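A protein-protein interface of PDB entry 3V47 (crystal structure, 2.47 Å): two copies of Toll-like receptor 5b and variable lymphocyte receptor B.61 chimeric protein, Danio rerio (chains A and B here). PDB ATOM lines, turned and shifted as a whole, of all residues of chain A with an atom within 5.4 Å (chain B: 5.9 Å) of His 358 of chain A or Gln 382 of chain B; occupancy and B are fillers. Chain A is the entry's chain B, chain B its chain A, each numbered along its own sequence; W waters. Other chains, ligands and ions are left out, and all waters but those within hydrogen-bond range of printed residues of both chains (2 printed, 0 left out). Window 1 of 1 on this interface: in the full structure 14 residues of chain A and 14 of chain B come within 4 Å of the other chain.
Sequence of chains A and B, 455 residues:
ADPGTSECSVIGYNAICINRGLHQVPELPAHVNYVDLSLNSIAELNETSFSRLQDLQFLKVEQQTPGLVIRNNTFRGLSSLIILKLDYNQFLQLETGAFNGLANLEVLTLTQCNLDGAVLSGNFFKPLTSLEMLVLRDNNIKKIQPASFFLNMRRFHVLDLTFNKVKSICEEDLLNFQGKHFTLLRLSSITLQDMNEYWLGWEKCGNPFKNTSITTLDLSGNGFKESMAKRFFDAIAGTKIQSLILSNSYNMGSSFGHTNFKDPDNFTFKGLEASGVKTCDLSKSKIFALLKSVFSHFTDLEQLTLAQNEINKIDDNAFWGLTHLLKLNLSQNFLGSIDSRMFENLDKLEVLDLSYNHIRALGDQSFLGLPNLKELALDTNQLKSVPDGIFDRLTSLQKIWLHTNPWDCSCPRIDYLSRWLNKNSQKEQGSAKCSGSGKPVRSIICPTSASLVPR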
ATOM      1  N   ASN A 333     -20.003  11.418 -20.404  1.00  0.00           N
ATOM      2  CA  ASN A 333     -20.164  11.707 -18.995  1.00  0.00           C
ATOM      3  C   ASN A 333     -19.244  10.777 -18.220  1.00  0.00           C
ATOM      4  O   ASN A 333     -18.305  10.277 -18.824  1.00  0.00           O
ATOM      5  CB  ASN A 333     -21.641  11.639 -18.629  1.00  0.00           C
ATOM      6  CG  ASN A 333     -22.335  12.954 -18.912  1.00  0.00           C
ATOM      7  OD1 ASN A 333     -22.026  13.945 -18.258  1.00  0.00           O
ATOM      8  ND2 ASN A 333     -23.263  12.985 -19.882  1.00  0.00           N
ATOM      9  N   PHE A 334     -19.503  10.535 -16.927  1.00  0.00           N
ATOM     10  CA  PHE A 334     -18.624   9.679 -16.109  1.00  0.00           C
ATOM     11  C   PHE A 334     -19.362   8.501 -15.437  1.00  0.00           C
ATOM     12  O   PHE A 334     -19.043   8.106 -14.321  1.00  0.00           O
ATOM     13  CB  PHE A 334     -17.949  10.520 -15.027  1.00  0.00           C
ATOM     14  CG  PHE A 334     -16.871  11.450 -15.550  1.00  0.00           C
ATOM     15  CD1 PHE A 334     -15.578  11.012 -15.736  1.00  0.00           C
ATOM     16  CD2 PHE A 334     -17.142  12.765 -15.824  1.00  0.00           C
ATOM     17  CE1 PHE A 334     -14.564  11.884 -16.226  1.00  0.00           C
ATOM     18  CE2 PHE A 334     -16.122  13.651 -16.308  1.00  0.00           C
ATOM     19  CZ  PHE A 334     -14.845  13.197 -16.499  1.00  0.00           C
ATOM     20  N   LEU A 335     -20.344   7.948 -16.110  1.00  0.00           N
ATOM     21  CA  LEU A 335     -21.137   6.874 -15.529  1.00  0.00           C
ATOM     22  C   LEU A 335     -20.273   5.637 -15.470  1.00  0.00           C
ATOM     23  O   LEU A 335     -19.624   5.300 -16.473  1.00  0.00           O
ATOM     24  CB  LEU A 335     -22.384   6.609 -16.397  1.00  0.00           C
ATOM     25  CG  LEU A 335     -23.465   7.688 -16.336  1.00  0.00           C
ATOM     26  CD1 LEU A 335     -24.598   7.402 -17.325  1.00  0.00           C
ATOM     27  CD2 LEU A 335     -24.056   7.768 -14.916  1.00  0.00           C
ATOM     28  N   GLY A 336     -20.255   4.963 -14.312  1.00  0.00           N
ATOM     29  CA  GLY A 336     -19.435   3.759 -14.146  1.00  0.00           C
ATOM     30  C   GLY A 336     -20.214   2.473 -14.295  1.00  0.00           C
ATOM     31  O   GLY A 336     -19.635   1.409 -14.546  1.00  0.00           O
ATOM     32  N   SER A 337     -21.532   2.579 -14.148  1.00  0.00           N
ATOM     33  CA  SER A 337     -22.427   1.435 -14.227  1.00  0.00           C
ATOM     34  C   SER A 337     -23.859   1.887 -14.440  1.00  0.00           C
ATOM     35  O   SER A 337     -24.176   3.080 -14.332  1.00  0.00           O
ATOM     36  CB  SER A 337     -22.331   0.540 -12.991  1.00  0.00           C
ATOM     37  OG  SER A 337     -22.591   1.265 -11.812  1.00  0.00           O
ATOM     38  N   TYR A 356     -19.362   6.910 -24.664  1.00  0.00           N
ATOM     39  CA  TYR A 356     -18.313   7.734 -24.087  1.00  0.00           C
ATOM     40  C   TYR A 356     -18.544   8.022 -22.595  1.00  0.00           C
ATOM     41  O   TYR A 356     -18.408   9.162 -22.125  1.00  0.00           O
ATOM     42  CB  TYR A 356     -18.175   9.042 -24.855  1.00  0.00           C
ATOM     43  CG  TYR A 356     -17.496   8.945 -26.193  1.00  0.00           C
ATOM     44  CD1 TYR A 356     -18.218   8.594 -27.343  1.00  0.00           C
ATOM     45  CD2 TYR A 356     -16.127   9.271 -26.332  1.00  0.00           C
ATOM     46  CE1 TYR A 356     -17.604   8.529 -28.600  1.00  0.00           C
ATOM     47  CE2 TYR A 356     -15.506   9.210 -27.586  1.00  0.00           C
ATOM     48  CZ  TYR A 356     -16.266   8.832 -28.706  1.00  0.00           C
ATOM     49  OH  TYR A 356     -15.665   8.765 -29.937  1.00  0.00           O
ATOM     50  N   ASN A 357     -18.881   6.988 -21.849  1.00  0.00           N
ATOM     51  CA  ASN A 357     -18.854   7.058 -20.410  1.00  0.00           C
ATOM     52  C   ASN A 357     -17.755   6.127 -19.917  1.00  0.00           C
ATOM     53  O   ASN A 357     -16.820   5.799 -20.643  1.00  0.00           O
ATOM     54  CB  ASN A 357     -20.234   6.655 -19.824  1.00  0.00           C
ATOM     55  CG  ASN A 357     -21.232   7.800 -19.857  1.00  0.00           C
ATOM     56  OD1 ASN A 357     -21.328   8.562 -18.902  1.00  0.00           O
ATOM     57  ND2 ASN A 357     -21.914   7.965 -20.968  1.00  0.00           N
ATOM     58  N   HIS A 358     -17.867   5.665 -18.689  1.00  0.00           N
ATOM     59  CA  HIS A 358     -16.828   4.777 -18.195  1.00  0.00           C
ATOM     60  C   HIS A 358     -17.516   3.549 -17.651  1.00  0.00           C
ATOM     61  O   HIS A 358     -17.154   3.016 -16.630  1.00  0.00           O
ATOM     62  CB  HIS A 358     -15.914   5.507 -17.186  1.00  0.00           C
ATOM     63  CG  HIS A 358     -15.273   6.758 -17.740  1.00  0.00           C
ATOM     64  ND1 HIS A 358     -14.565   6.778 -18.929  1.00  0.00           N
ATOM     65  CD2 HIS A 358     -15.191   8.021 -17.243  1.00  0.00           C
ATOM     66  CE1 HIS A 358     -14.102   7.997 -19.150  1.00  0.00           C
ATOM     67  NE2 HIS A 358     -14.475   8.771 -18.146  1.00  0.00           N
ATOM     68  N   ILE A 359     -18.537   3.104 -18.366  1.00  0.00           N
ATOM     69  CA  ILE A 359     -19.408   2.044 -17.885  1.00  0.00           C
ATOM     70  C   ILE A 359     -18.699   0.710 -17.852  1.00  0.00           C
ATOM     71  O   ILE A 359     -18.239   0.232 -18.847  1.00  0.00           O
ATOM     72  CB  ILE A 359     -20.723   1.992 -18.695  1.00  0.00           C
ATOM     73  CG1 ILE A 359     -21.547   3.258 -18.413  1.00  0.00           C
ATOM     74  CG2 ILE A 359     -21.548   0.717 -18.374  1.00  0.00           C
ATOM     75  CD1 ILE A 359     -22.699   3.509 -19.388  1.00  0.00           C
ATOM     76  N   ARG A 360     -18.599   0.122 -16.680  1.00  0.00           N
ATOM     77  CA  ARG A 360     -17.891  -1.127 -16.524  1.00  0.00           C
ATOM     78  C   ARG A 360     -18.869  -2.246 -16.254  1.00  0.00           C
ATOM     79  O   ARG A 360     -18.490  -3.418 -16.281  1.00  0.00           O
ATOM     80  CB  ARG A 360     -16.897  -1.038 -15.368  1.00  0.00           C
ATOM     81  CG  ARG A 360     -15.580  -0.431 -15.806  1.00  0.00           C
ATOM     82  CD  ARG A 360     -14.658  -0.159 -14.636  1.00  0.00           C
ATOM     83  NE  ARG A 360     -13.413   0.446 -15.104  1.00  0.00           N
ATOM     84  CZ  ARG A 360     -12.476   0.932 -14.295  1.00  0.00           C
ATOM     85  NH1 ARG A 360     -12.661   0.863 -12.982  1.00  0.00           N
ATOM     86  NH2 ARG A 360     -11.356   1.458 -14.789  1.00  0.00           N
ATOM     87  N   THR A 380     -18.002   2.707 -26.745  1.00  0.00           N
ATOM     88  CA  THR A 380     -16.990   3.548 -26.142  1.00  0.00           C
ATOM     89  C   THR A 380     -17.280   3.640 -24.659  1.00  0.00           C
ATOM     90  O   THR A 380     -17.521   4.720 -24.094  1.00  0.00           O
ATOM     91  CB  THR A 380     -16.997   4.952 -26.803  1.00  0.00           C
ATOM     92  OG1 THR A 380     -17.199   4.802 -28.228  1.00  0.00           O
ATOM     93  CG2 THR A 380     -15.679   5.694 -26.507  1.00  0.00           C
ATOM     94  N   ASN A 381     -17.288   2.486 -24.026  1.00  0.00           N
ATOM     95  CA  ASN A 381     -17.437   2.448 -22.607  1.00  0.00           C
ATOM     96  C   ASN A 381     -16.344   1.489 -22.131  1.00  0.00           C
ATOM     97  O   ASN A 381     -15.278   1.448 -22.747  1.00  0.00           O
ATOM     98  CB  ASN A 381     -18.864   2.052 -22.244  1.00  0.00           C
ATOM     99  CG  ASN A 381     -19.751   3.259 -22.034  1.00  0.00           C
ATOM    100  OD1 ASN A 381     -19.472   4.097 -21.166  1.00  0.00           O
ATOM    101  ND2 ASN A 381     -20.790   3.388 -22.841  1.00  0.00           N
ATOM    102  N   GLN A 382     -16.587   0.704 -21.078  1.00  0.00           N
ATOM    103  CA  GLN A 382     -15.559  -0.204 -20.654  1.00  0.00           C
ATOM    104  C   GLN A 382     -16.186  -1.504 -20.221  1.00  0.00           C
ATOM    105  O   GLN A 382     -15.847  -2.049 -19.169  1.00  0.00           O
ATOM    106  CB  GLN A 382     -14.693   0.432 -19.548  1.00  0.00           C
ATOM    107  CG  GLN A 382     -13.363  -0.265 -19.366  1.00  0.00           C
ATOM    108  CD  GLN A 382     -12.403   0.478 -18.473  1.00  0.00           C
ATOM    109  OE1 GLN A 382     -12.276   0.157 -17.271  1.00  0.00           O
ATOM    110  NE2 GLN A 382     -11.676   1.461 -19.056  1.00  0.00           N
ATOM    111  N   ASN B 357      -8.245   2.466 -17.955  1.00  0.00           N
ATOM    112  CA  ASN B 357      -8.487   3.647 -17.172  1.00  0.00           C
ATOM    113  C   ASN B 357      -9.566   4.421 -17.867  1.00  0.00           C
ATOM    114  O   ASN B 357     -10.360   3.856 -18.623  1.00  0.00           O
ATOM    115  CB  ASN B 357      -7.205   4.443 -16.927  1.00  0.00           C
ATOM    116  CG  ASN B 357      -6.353   3.819 -15.849  1.00  0.00           C
ATOM    117  OD1 ASN B 357      -6.448   4.211 -14.695  1.00  0.00           O
ATOM    118  ND2 ASN B 357      -5.561   2.796 -16.201  1.00  0.00           N
ATOM    119  N   HIS B 358      -9.633   5.714 -17.600  1.00  0.00           N
ATOM    120  CA  HIS B 358     -10.579   6.521 -18.305  1.00  0.00           C
ATOM    121  C   HIS B 358      -9.851   7.658 -19.024  1.00  0.00           C
ATOM    122  O   HIS B 358     -10.308   8.788 -19.056  1.00  0.00           O
ATOM    123  CB  HIS B 358     -11.668   6.962 -17.322  1.00  0.00           C
ATOM    124  CG  HIS B 358     -12.357   5.804 -16.635  1.00  0.00           C
ATOM    125  ND1 HIS B 358     -12.844   4.703 -17.325  1.00  0.00           N
ATOM    126  CD2 HIS B 358     -12.691   5.600 -15.331  1.00  0.00           C
ATOM    127  CE1 HIS B 358     -13.419   3.867 -16.481  1.00  0.00           C
ATOM    128  NE2 HIS B 358     -13.337   4.385 -15.267  1.00  0.00           N
ATOM    129  N   ILE B 359      -8.708   7.336 -19.618  1.00  0.00           N
ATOM    130  CA  ILE B 359      -7.786   8.361 -20.101  1.00  0.00           C
ATOM    131  C   ILE B 359      -8.353   9.018 -21.341  1.00  0.00           C
ATOM    132  O   ILE B 359      -8.676   8.356 -22.333  1.00  0.00           O
ATOM    133  CB  ILE B 359      -6.383   7.788 -20.332  1.00  0.00           C
ATOM    134  CG1 ILE B 359      -5.784   7.351 -18.978  1.00  0.00           C
ATOM    135  CG2 ILE B 359      -5.481   8.830 -21.052  1.00  0.00           C
ATOM    136  CD1 ILE B 359      -4.404   6.639 -19.089  1.00  0.00           C
ATOM    137  N   ARG B 360      -8.529  10.326 -21.258  1.00  0.00           N
ATOM    138  CA  ARG B 360      -9.120  11.053 -22.345  1.00  0.00           C
ATOM    139  C   ARG B 360      -8.097  11.896 -23.045  1.00  0.00           C
ATOM    140  O   ARG B 360      -8.346  12.363 -24.145  1.00  0.00           O
ATOM    141  CB  ARG B 360     -10.280  11.920 -21.860  1.00  0.00           C
ATOM    142  CG  ARG B 360     -11.612  11.253 -22.059  1.00  0.00           C
ATOM    143  CD  ARG B 360     -12.703  11.916 -21.216  1.00  0.00           C
ATOM    144  NE  ARG B 360     -13.934  11.123 -21.162  1.00  0.00           N
ATOM    145  CZ  ARG B 360     -15.044  11.485 -20.494  1.00  0.00           C
ATOM    146  NH1 ARG B 360     -15.046  12.618 -19.799  1.00  0.00           N
ATOM    147  NH2 ARG B 360     -16.157  10.719 -20.513  1.00  0.00           N
ATOM    148  N   ALA B 361      -6.945  12.099 -22.405  1.00  0.00           N
ATOM    149  CA  ALA B 361      -5.916  12.941 -22.991  1.00  0.00           C
ATOM    150  C   ALA B 361      -4.541  12.529 -22.497  1.00  0.00           C
ATOM    151  O   ALA B 361      -4.372  12.224 -21.313  1.00  0.00           O
ATOM    152  CB  ALA B 361      -6.188  14.452 -22.677  1.00  0.00           C
ATOM    153  N   THR B 380      -7.897   0.284 -24.197  1.00  0.00           N
ATOM    154  CA  THR B 380      -9.081   0.284 -23.377  1.00  0.00           C
ATOM    155  C   THR B 380      -9.059   1.538 -22.516  1.00  0.00           C
ATOM    156  O   THR B 380      -9.101   1.498 -21.301  1.00  0.00           O
ATOM    157  CB  THR B 380      -9.128  -0.993 -22.538  1.00  0.00           C
ATOM    158  OG1 THR B 380      -8.671  -2.097 -23.358  1.00  0.00           O
ATOM    159  CG2 THR B 380     -10.501  -1.240 -22.015  1.00  0.00           C
ATOM    160  N   ASN B 381      -8.993   2.667 -23.181  1.00  0.00           N
ATOM    161  CA  ASN B 381      -9.130   3.919 -22.491  1.00  0.00           C
ATOM    162  C   ASN B 381     -10.153   4.712 -23.291  1.00  0.00           C
ATOM    163  O   ASN B 381     -11.050   4.116 -23.840  1.00  0.00           O
ATOM    164  CB  ASN B 381      -7.769   4.577 -22.364  1.00  0.00           C
ATOM    165  CG  ASN B 381      -7.051   4.155 -21.077  1.00  0.00           C
ATOM    166  OD1 ASN B 381      -7.442   4.564 -19.992  1.00  0.00           O
ATOM    167  ND2 ASN B 381      -6.016   3.338 -21.197  1.00  0.00           N
ATOM    168  N   GLN B 382     -10.041   6.031 -23.370  1.00  0.00           N
ATOM    169  CA  GLN B 382     -10.997   6.781 -24.154  1.00  0.00           C
ATOM    170  C   GLN B 382     -10.280   7.852 -24.958  1.00  0.00           C
ATOM    171  O   GLN B 382     -10.671   9.008 -24.991  1.00  0.00           O
ATOM    172  CB  GLN B 382     -12.100   7.339 -23.262  1.00  0.00           C
ATOM    173  CG  GLN B 382     -13.385   7.711 -24.009  1.00  0.00           C
ATOM    174  CD  GLN B 382     -14.537   8.014 -23.041  1.00  0.00           C
ATOM    175  OE1 GLN B 382     -14.792   9.171 -22.742  1.00  0.00           O
ATOM    176  NE2 GLN B 382     -15.208   6.965 -22.525  1.00  0.00           N
ATOM    177  N   LEU B 383      -9.241   7.448 -25.659  1.00  0.00           N
ATOM    178  CA  LEU B 383      -8.428   8.414 -26.363  1.00  0.00           C
ATOM    179  C   LEU B 383      -8.932   8.650 -27.756  1.00  0.00           C
ATOM    180  O   LEU B 383      -9.137   7.714 -28.513  1.00  0.00           O
ATOM    181  CB  LEU B 383      -6.973   7.975 -26.389  1.00  0.00           C
ATOM    182  CG  LEU B 383      -6.262   8.121 -25.049  1.00  0.00           C
ATOM    183  CD1 LEU B 383      -5.031   7.216 -24.979  1.00  0.00           C
ATOM    184  CD2 LEU B 383      -5.888   9.578 -24.811  1.00  0.00           C
ATOM    185  N   LYS B 384      -9.135   9.919 -28.092  1.00  0.00           N
ATOM    186  CA  LYS B 384      -9.520  10.245 -29.428  1.00  0.00           C
ATOM    187  C   LYS B 384      -8.293  10.496 -30.229  1.00  0.00           C
ATOM    188  O   LYS B 384      -8.293  10.270 -31.428  1.00  0.00           O
ATOM    189  CB  LYS B 384     -10.446  11.454 -29.460  1.00  0.00           C
ATOM    190  CG  LYS B 384     -11.896  11.120 -29.144  1.00  0.00           C
ATOM    191  CD  LYS B 384     -12.613  12.396 -28.735  1.00  0.00           C
ATOM    192  CE  LYS B 384     -14.021  12.419 -29.275  1.00  0.00           C
ATOM    193  NZ  LYS B 384     -14.986  12.837 -28.188  1.00  0.00           N
ATOM    194  N   THR B 404      -9.033  -0.494 -28.782  1.00  0.00           N
ATOM    195  CA  THR B 404     -10.203  -0.206 -27.923  1.00  0.00           C
ATOM    196  C   THR B 404     -10.117   1.239 -27.354  1.00  0.00           C
ATOM    197  O   THR B 404     -10.338   1.501 -26.172  1.00  0.00           O
ATOM    198  CB  THR B 404     -10.387  -1.326 -26.830  1.00  0.00           C
ATOM    199  OG1 THR B 404      -9.998  -2.587 -27.389  1.00  0.00           O
ATOM    200  CG2 THR B 404     -11.818  -1.461 -26.363  1.00  0.00           C
ATOM    201  N   ASN B 405      -9.768   2.171 -28.235  1.00  0.00           N
ATOM    202  CA  ASN B 405      -9.888   3.571 -27.954  1.00  0.00           C
ATOM    203  C   ASN B 405     -10.629   4.114 -29.159  1.00  0.00           C
ATOM    204  O   ASN B 405     -10.472   3.574 -30.237  1.00  0.00           O
ATOM    205  CB  ASN B 405      -8.496   4.201 -27.840  1.00  0.00           C
ATOM    206  CG  ASN B 405      -7.913   4.044 -26.460  1.00  0.00           C
ATOM    207  OD1 ASN B 405      -8.446   4.608 -25.487  1.00  0.00           O
ATOM    208  ND2 ASN B 405      -6.833   3.263 -26.352  1.00  0.00           N
ATOM    209  N   PRO B 406     -11.454   5.162 -28.981  1.00  0.00           N
ATOM    210  CA  PRO B 406     -12.193   5.777 -30.100  1.00  0.00           C
ATOM    211  C   PRO B 406     -11.303   6.685 -30.963  1.00  0.00           C
ATOM    212  O   PRO B 406     -11.495   7.902 -30.977  1.00  0.00           O
ATOM    213  CB  PRO B 406     -13.231   6.628 -29.374  1.00  0.00           C
ATOM    214  CG  PRO B 406     -12.497   7.054 -28.108  1.00  0.00           C
ATOM    215  CD  PRO B 406     -11.706   5.860 -27.709  1.00  0.00           C
HETATM  216  O   HOH W   1     -13.887   3.853 -24.031  1.00  0.00           O
HETATM  217  O   HOH W   2     -12.057  10.413 -17.663  1.00  0.00           O
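Water W2 lies within hydrogen-bond range of the backbone carbonyl oxygen of His 358 of chain B and a ring nitrogen (NE2) of His 358 of chain A.
Water W1 lies within hydrogen-bond range of O of Asn 381 of chain B (2.9 Å) and O of Asn 381 of chain A (3.1 Å).
The guanidinium group (NE) of Arg 360 of chain A is in hydrogen-bond range of the side-chain amide oxygen (OE1) of Gln 382 of chain A, at 2.5 Å.
The backbone NH (N) of Thr 380 of chain B lies close to the backbone carbonyl oxygen (O) of Thr 404 of chain B (3.4 Å).
The side-chain amide oxygen of Asn 381 of chain B lies close to the backbone NH of Asn 357 of chain B, at 3.0 Å.
The backbone carbonyl oxygen (O) of Ile 359 of chain B is in hydrogen-bond range of the backbone NH (N) of Gln 382 of chain B (2.9 Å).
The side-chain amide oxygen of Asn 357 of chain A lies within hydrogen-bond range of the backbone NH of Phe 334 of chain A (3.3 Å).
N of Gln 382 of chain A sits at hydrogen-bond distance from O of Ile 359 of chain A.
Hydrophobic or aromatic side chains of chain B within 4 Å of the printed part of chain A: His 358 and Pro 406.
Along chain B the printed residues that touch a printed residue of chain A span positions 357 to 406.
Printed residues of chain A that touch a printed residue of chain B: Asn 333, Phe 334, Tyr 356, Asn 357, His 358, Arg 360, Thr 380 and Gln 382.
Among the printed residues, 16 pairs touch across the chains.
Arg 360 of chain B touches Phe 334 of chain A.
Tyr 356 of chain A touches Gln 382 of chain B (C to NE2, 3.5 Å).
Tyr 356 of chain A touches Lys 384 of chain B (CE2 to NZ, 3.7 Å).
Tyr 356 of chain A touches Pro 406 of chain B (OH to CB, 3.3 Å).
Gln 382 of chain B touches His 358 of chain A.
Arg 360 of chain A touches His 358 of chain B (NH2 to NE2, 3.6 Å).
Gln 382 of chain B touches Thr 380 of chain A (NE2 to O, 3.6 Å).
CG2 of Thr 380 of chain A touches CG of Pro 406 of chain B, 3.8 Å away.
His 358 of chain B touches Gln 382 of chain A (ND1 to NE2, 3.9 Å).
Asn 357 of chain A touches Gln 382 of chain B, and with the chains exchanged Gln 382 of chain A touches Asn 357 of chain B.
His 358 of chain B touches its own counterpart, His 358 of chain A.
His 358 of chain A touches Arg 360 of chain B, and with the chains exchanged Arg 360 of chain A touches His 358 of chain B.
Thr 380 of chain A touches Gln 382 of chain B, and with the chains exchanged Gln 382 of chain A touches Thr 380 of chain B.
Positions printed for both chains: 357, 358, 359, 360, 380, 381 and 382.
His 358 of chain A touches just these residues of chain B: His 358, Arg 360 and Gln 382.
Gln 382 of chain B touches four residues of chain A.
Printed residues of chain B within 4 Å of Asn 333 of chain A: Arg 360 (2.8 Å).
Printed residues of chain A within 4 Å of Pro 406 of chain B: Tyr 356 and Thr 380.
Printed residues of chain B within 4 Å of Tyr 356 of chain A: Arg 360, Gln 382, Lys 384 and Pro 406.
Printed residues of chain A within 4 Å of Arg 360 of chain B: Asn 333 (2.8 Å), Phe 334 (3.4 Å), Tyr 356 (3.2 Å) and His 358 (3.5 Å).
Of the printed residues of chain A, Asn 357 of chain B touches Gln 382 (2.8 Å).
The nearest residue of chain A that does not touch Gln 382 of chain B is Asn 381 of chain A (5.0 Å).
The nearest printed residue of chain A that does not touch Thr 380 of chain B is Asn 381 of chain A (5.5 Å).
The side-chain amide nitrogen (NE2) of Gln 382 of chain A lies within hydrogen-bond range of the backbone carbonyl oxygen (O) of Thr 380 of chain B, 3.4 Å away.
NH2 of Arg 360 of chain B is in hydrogen-bond range of O of Asn 333 of chain A (2.8 Å).
The guanidinium group (NH2) of Arg 360 of chain B lies within hydrogen-bond range of a ring nitrogen (NE2) of His 358 of chain A, 3.5 Å away.
A ring nitrogen (ND1) of His 358 of chain B lies within hydrogen-bond range of a ring nitrogen (ND1) of His 358 of chain A (3.1 Å).
The backbone carbonyl oxygen (O) of Asn 357 of chain A is in hydrogen-bond range of the side-chain amide nitrogen (NE2) of Gln 382 of chain B (2.7 Å).
The guanidinium group (NH2) of Arg 360 of chain B lies within hydrogen-bond range of the backbone carbonyl oxygen (O) of Tyr 356 of chain A (3.2 Å).
NE2 of Gln 382 of chain A sits at hydrogen-bond distance from O of Asn 357 of chain B (2.8 Å).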
